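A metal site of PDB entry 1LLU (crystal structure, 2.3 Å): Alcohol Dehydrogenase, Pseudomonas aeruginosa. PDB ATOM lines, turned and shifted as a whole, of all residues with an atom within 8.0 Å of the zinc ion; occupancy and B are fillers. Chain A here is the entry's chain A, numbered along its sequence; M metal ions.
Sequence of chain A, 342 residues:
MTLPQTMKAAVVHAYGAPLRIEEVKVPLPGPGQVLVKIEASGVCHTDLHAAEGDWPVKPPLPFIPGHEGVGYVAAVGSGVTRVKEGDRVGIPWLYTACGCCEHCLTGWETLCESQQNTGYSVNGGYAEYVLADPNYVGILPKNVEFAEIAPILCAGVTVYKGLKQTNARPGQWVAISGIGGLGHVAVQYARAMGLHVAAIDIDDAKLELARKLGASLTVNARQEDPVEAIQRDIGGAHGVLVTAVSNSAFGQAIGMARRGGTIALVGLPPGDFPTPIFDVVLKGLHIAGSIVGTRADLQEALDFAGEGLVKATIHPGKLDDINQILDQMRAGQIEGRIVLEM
The zinc ion is bound by the side-chain sulfur of Cys 112 (2.4 Å), the side-chain sulfur of Cys 104 (2.4 Å), the side-chain sulfur of Cys 98 (2.5 Å) and the side-chain sulfur of Cys 101 (2.6 Å).
N of Gly 99 touches the zinc ion, 3.8 Å away.
Within 4 Å of the zinc ion: Cys 98, Gly 99, Cys 101, Cys 104 and Cys 112.
O of Cys 112 lies within hydrogen-bond range of NE2 of Gln 115.
The side-chain sulfur (SG) of Cys 104 sits close to the backbone NH (N) of Gly 99.
N of Ser 114 lies close to SG of Cys 112 (3.3 Å).
The side-chain sulfur of Cys 98 lies close to the backbone NH of Cys 100.
SG of Cys 101 lies close to N of His 103 (3.5 Å).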
ATOM      1  N   THR A  96      -3.462  15.749 -25.886  1.00  0.00           N
ATOM      2  CA  THR A  96      -3.980  15.885 -24.531  1.00  0.00           C
ATOM      3  C   THR A  96      -5.059  16.962 -24.547  1.00  0.00           C
ATOM      4  O   THR A  96      -5.251  17.627 -25.552  1.00  0.00           O
ATOM      5  CB  THR A  96      -2.827  16.263 -23.539  1.00  0.00           C
ATOM      6  OG1 THR A  96      -3.298  16.167 -22.184  1.00  0.00           O
ATOM      7  CG2 THR A  96      -2.336  17.684 -23.789  1.00  0.00           C
ATOM      8  N   ALA A  97      -5.769  17.102 -23.423  1.00  0.00           N
ATOM      9  CA  ALA A  97      -6.833  18.097 -23.259  1.00  0.00           C
ATOM     10  C   ALA A  97      -6.950  18.291 -21.748  1.00  0.00           C
ATOM     11  O   ALA A  97      -6.523  17.418 -20.990  1.00  0.00           O
ATOM     12  CB  ALA A  97      -8.150  17.592 -23.853  1.00  0.00           C
ATOM     13  N   CYS A  98      -7.529  19.400 -21.295  1.00  0.00           N
ATOM     14  CA  CYS A  98      -7.624  19.659 -19.857  1.00  0.00           C
ATOM     15  C   CYS A  98      -8.550  18.739 -19.067  1.00  0.00           C
ATOM     16  O   CYS A  98      -8.304  18.473 -17.897  1.00  0.00           O
ATOM     17  CB  CYS A  98      -7.982  21.135 -19.587  1.00  0.00           C
ATOM     18  SG  CYS A  98      -9.713  21.644 -19.772  1.00  0.00           S
ATOM     19  N   GLY A  99      -9.602  18.250 -19.705  1.00  0.00           N
ATOM     20  CA  GLY A  99     -10.513  17.342 -19.040  1.00  0.00           C
ATOM     21  C   GLY A  99     -11.593  17.949 -18.152  1.00  0.00           C
ATOM     22  O   GLY A  99     -12.406  17.209 -17.594  1.00  0.00           O
ATOM     23  N   CYS A 100     -11.631  19.265 -18.013  1.00  0.00           N
ATOM     24  CA  CYS A 100     -12.652  19.855 -17.169  1.00  0.00           C
ATOM     25  C   CYS A 100     -13.280  21.169 -17.636  1.00  0.00           C
ATOM     26  O   CYS A 100     -13.850  21.900 -16.836  1.00  0.00           O
ATOM     27  CB  CYS A 100     -12.116  20.019 -15.738  1.00  0.00           C
ATOM     28  SG  CYS A 100     -10.547  20.871 -15.608  1.00  0.00           S
ATOM     29  N   CYS A 101     -13.193  21.456 -18.928  1.00  0.00           N
ATOM     30  CA  CYS A 101     -13.794  22.667 -19.471  1.00  0.00           C
ATOM     31  C   CYS A 101     -15.120  22.268 -20.117  1.00  0.00           C
ATOM     32  O   CYS A 101     -15.434  21.089 -20.196  1.00  0.00           O
ATOM     33  CB  CYS A 101     -12.875  23.309 -20.523  1.00  0.00           C
ATOM     34  SG  CYS A 101     -12.850  22.454 -22.129  1.00  0.00           S
ATOM     35  N   GLU A 102     -15.884  23.268 -20.578  1.00  0.00           N
ATOM     36  CA  GLU A 102     -17.172  23.060 -21.233  1.00  0.00           C
ATOM     37  C   GLU A 102     -17.151  21.901 -22.227  1.00  0.00           C
ATOM     38  O   GLU A 102     -17.986  21.001 -22.185  1.00  0.00           O
ATOM     39  CB  GLU A 102     -17.565  24.286 -22.050  1.00  0.00           C
ATOM     40  CG  GLU A 102     -18.096  25.462 -21.294  1.00  0.00           C
ATOM     41  CD  GLU A 102     -18.761  26.443 -22.233  1.00  0.00           C
ATOM     42  OE1 GLU A 102     -19.438  27.378 -21.740  1.00  0.00           O
ATOM     43  OE2 GLU A 102     -18.614  26.286 -23.465  1.00  0.00           O
ATOM     44  N   HIS A 103     -16.181  21.970 -23.138  1.00  0.00           N
ATOM     45  CA  HIS A 103     -16.011  20.996 -24.209  1.00  0.00           C
ATOM     46  C   HIS A 103     -15.616  19.619 -23.735  1.00  0.00           C
ATOM     47  O   HIS A 103     -16.204  18.631 -24.163  1.00  0.00           O
ATOM     48  CB  HIS A 103     -15.002  21.534 -25.217  1.00  0.00           C
ATOM     49  CG  HIS A 103     -15.272  22.957 -25.613  1.00  0.00           C
ATOM     50  ND1 HIS A 103     -16.430  23.350 -26.236  1.00  0.00           N
ATOM     51  CD2 HIS A 103     -14.567  24.099 -25.386  1.00  0.00           C
ATOM     52  CE1 HIS A 103     -16.442  24.664 -26.374  1.00  0.00           C
ATOM     53  NE2 HIS A 103     -15.317  25.147 -25.855  1.00  0.00           N
ATOM     54  N   CYS A 104     -14.611  19.554 -22.874  1.00  0.00           N
ATOM     55  CA  CYS A 104     -14.129  18.283 -22.347  1.00  0.00           C
ATOM     56  C   CYS A 104     -15.223  17.543 -21.570  1.00  0.00           C
ATOM     57  O   CYS A 104     -15.346  16.314 -21.668  1.00  0.00           O
ATOM     58  CB  CYS A 104     -12.907  18.510 -21.447  1.00  0.00           C
ATOM     59  SG  CYS A 104     -11.355  18.746 -22.365  1.00  0.00           S
ATOM     60  N   LEU A 105     -16.026  18.286 -20.809  1.00  0.00           N
ATOM     61  CA  LEU A 105     -17.083  17.687 -19.999  1.00  0.00           C
ATOM     62  C   LEU A 105     -18.339  17.284 -20.778  1.00  0.00           C
ATOM     63  O   LEU A 105     -19.163  16.531 -20.271  1.00  0.00           O
ATOM     64  CB  LEU A 105     -17.462  18.621 -18.857  1.00  0.00           C
ATOM     65  CG  LEU A 105     -16.356  18.879 -17.817  1.00  0.00           C
ATOM     66  CD1 LEU A 105     -16.831  19.916 -16.812  1.00  0.00           C
ATOM     67  CD2 LEU A 105     -15.974  17.576 -17.130  1.00  0.00           C
ATOM     68  N   TRP A 108     -16.758  16.735 -26.098  1.00  0.00           N
ATOM     69  CA  TRP A 108     -16.102  17.494 -27.177  1.00  0.00           C
ATOM     70  C   TRP A 108     -14.690  17.940 -26.811  1.00  0.00           C
ATOM     71  O   TRP A 108     -14.330  19.095 -27.069  1.00  0.00           O
ATOM     72  CB  TRP A 108     -16.920  18.751 -27.528  1.00  0.00           C
ATOM     73  CG  TRP A 108     -18.123  18.464 -28.377  1.00  0.00           C
ATOM     74  CD1 TRP A 108     -19.382  18.154 -27.942  1.00  0.00           C
ATOM     75  CD2 TRP A 108     -18.135  18.321 -29.801  1.00  0.00           C
ATOM     76  NE1 TRP A 108     -20.172  17.818 -29.016  1.00  0.00           N
ATOM     77  CE2 TRP A 108     -19.437  17.904 -30.169  1.00  0.00           C
ATOM     78  CE3 TRP A 108     -17.173  18.487 -30.817  1.00  0.00           C
ATOM     79  CZ2 TRP A 108     -19.811  17.666 -31.508  1.00  0.00           C
ATOM     80  CZ3 TRP A 108     -17.544  18.247 -32.142  1.00  0.00           C
ATOM     81  CH2 TRP A 108     -18.848  17.831 -32.473  1.00  0.00           C
ATOM     82  N   GLU A 109     -13.875  17.053 -26.231  1.00  0.00           N
ATOM     83  CA  GLU A 109     -12.504  17.428 -25.833  1.00  0.00           C
ATOM     84  C   GLU A 109     -11.729  17.920 -27.045  1.00  0.00           C
ATOM     85  O   GLU A 109     -10.688  18.576 -26.946  1.00  0.00           O
ATOM     86  CB  GLU A 109     -11.774  16.229 -25.197  1.00  0.00           C
ATOM     87  CG  GLU A 109     -11.565  15.056 -26.107  1.00  0.00           C
ATOM     88  CD  GLU A 109     -12.387  13.857 -25.683  1.00  0.00           C
ATOM     89  OE1 GLU A 109     -13.611  14.044 -25.465  1.00  0.00           O
ATOM     90  OE2 GLU A 109     -11.837  12.754 -25.564  1.00  0.00           O
ATOM     91  N   THR A 110     -12.268  17.576 -28.208  1.00  0.00           N
ATOM     92  CA  THR A 110     -11.725  17.939 -29.491  1.00  0.00           C
ATOM     93  C   THR A 110     -11.633  19.474 -29.683  1.00  0.00           C
ATOM     94  O   THR A 110     -10.758  19.981 -30.399  1.00  0.00           O
ATOM     95  CB  THR A 110     -12.619  17.256 -30.563  1.00  0.00           C
ATOM     96  OG1 THR A 110     -11.876  16.203 -31.200  1.00  0.00           O
ATOM     97  CG2 THR A 110     -13.135  18.235 -31.554  1.00  0.00           C
ATOM     98  N   LEU A 111     -12.526  20.194 -29.017  1.00  0.00           N
ATOM     99  CA  LEU A 111     -12.594  21.648 -29.096  1.00  0.00           C
ATOM    100  C   LEU A 111     -11.899  22.328 -27.918  1.00  0.00           C
ATOM    101  O   LEU A 111     -11.982  23.552 -27.758  1.00  0.00           O
ATOM    102  CB  LEU A 111     -14.049  22.102 -29.142  1.00  0.00           C
ATOM    103  CG  LEU A 111     -14.961  21.478 -30.214  1.00  0.00           C
ATOM    104  CD1 LEU A 111     -16.394  21.960 -30.002  1.00  0.00           C
ATOM    105  CD2 LEU A 111     -14.451  21.847 -31.607  1.00  0.00           C
ATOM    106  N   CYS A 112     -11.224  21.535 -27.087  1.00  0.00           N
ATOM    107  CA  CYS A 112     -10.508  22.063 -25.919  1.00  0.00           C
ATOM    108  C   CYS A 112      -9.429  23.082 -26.282  1.00  0.00           C
ATOM    109  O   CYS A 112      -8.560  22.824 -27.130  1.00  0.00           O
ATOM    110  CB  CYS A 112      -9.890  20.922 -25.117  1.00  0.00           C
ATOM    111  SG  CYS A 112      -9.046  21.490 -23.616  1.00  0.00           S
ATOM    112  N   GLU A 113      -9.467  24.232 -25.624  1.00  0.00           N
ATOM    113  CA  GLU A 113      -8.477  25.278 -25.883  1.00  0.00           C
ATOM    114  C   GLU A 113      -7.117  25.010 -25.249  1.00  0.00           C
ATOM    115  O   GLU A 113      -6.131  25.659 -25.587  1.00  0.00           O
ATOM    116  CB  GLU A 113      -9.011  26.625 -25.403  1.00  0.00           C
ATOM    117  CG  GLU A 113     -10.351  27.001 -25.978  1.00  0.00           C
ATOM    118  CD  GLU A 113     -10.741  28.428 -25.673  1.00  0.00           C
ATOM    119  OE1 GLU A 113     -11.916  28.790 -25.874  1.00  0.00           O
ATOM    120  OE2 GLU A 113      -9.855  29.196 -25.237  1.00  0.00           O
ATOM    121  N   SER A 114      -7.058  24.054 -24.329  1.00  0.00           N
ATOM    122  CA  SER A 114      -5.821  23.707 -23.633  1.00  0.00           C
ATOM    123  C   SER A 114      -5.193  22.433 -24.185  1.00  0.00           C
ATOM    124  O   SER A 114      -4.349  21.811 -23.525  1.00  0.00           O
ATOM    125  CB  SER A 114      -6.100  23.512 -22.138  1.00  0.00           C
ATOM    126  OG  SER A 114      -6.668  24.670 -21.568  1.00  0.00           O
ATOM    127  N   GLN A 115      -5.589  22.040 -25.386  1.00  0.00           N
ATOM    128  CA  GLN A 115      -5.043  20.826 -25.968  1.00  0.00           C
ATOM    129  C   GLN A 115      -3.661  21.062 -26.581  1.00  0.00           C
ATOM    130  O   GLN A 115      -3.233  22.198 -26.775  1.00  0.00           O
ATOM    131  CB  GLN A 115      -5.983  20.307 -27.067  1.00  0.00           C
ATOM    132  CG  GLN A 115      -6.222  21.317 -28.190  1.00  0.00           C
ATOM    133  CD  GLN A 115      -7.101  20.779 -29.319  1.00  0.00           C
ATOM    134  OE1 GLN A 115      -6.625  20.104 -30.236  1.00  0.00           O
ATOM    135  NE2 GLN A 115      -8.386  21.077 -29.237  1.00  0.00           N
ATOM    136  N   TYR A 136      -5.004   9.928 -23.735  1.00  0.00           N
ATOM    137  CA  TYR A 136      -5.528  10.309 -25.032  1.00  0.00           C
ATOM    138  C   TYR A 136      -5.033   9.459 -26.176  1.00  0.00           C
ATOM    139  O   TYR A 136      -5.394   9.669 -27.332  1.00  0.00           O
ATOM    140  CB  TYR A 136      -5.223  11.776 -25.287  1.00  0.00           C
ATOM    141  CG  TYR A 136      -5.976  12.653 -24.321  1.00  0.00           C
ATOM    142  CD1 TYR A 136      -5.519  12.823 -23.004  1.00  0.00           C
ATOM    143  CD2 TYR A 136      -7.195  13.232 -24.677  1.00  0.00           C
ATOM    144  CE1 TYR A 136      -6.272  13.537 -22.068  1.00  0.00           C
ATOM    145  CE2 TYR A 136      -7.951  13.949 -23.754  1.00  0.00           C
ATOM    146  CZ  TYR A 136      -7.481  14.094 -22.452  1.00  0.00           C
ATOM    147  OH  TYR A 136      -8.229  14.804 -21.539  1.00  0.00           O
HETATM  148 ZN    ZN M   1     -10.720  21.020 -21.983  1.00  0.00          ZN
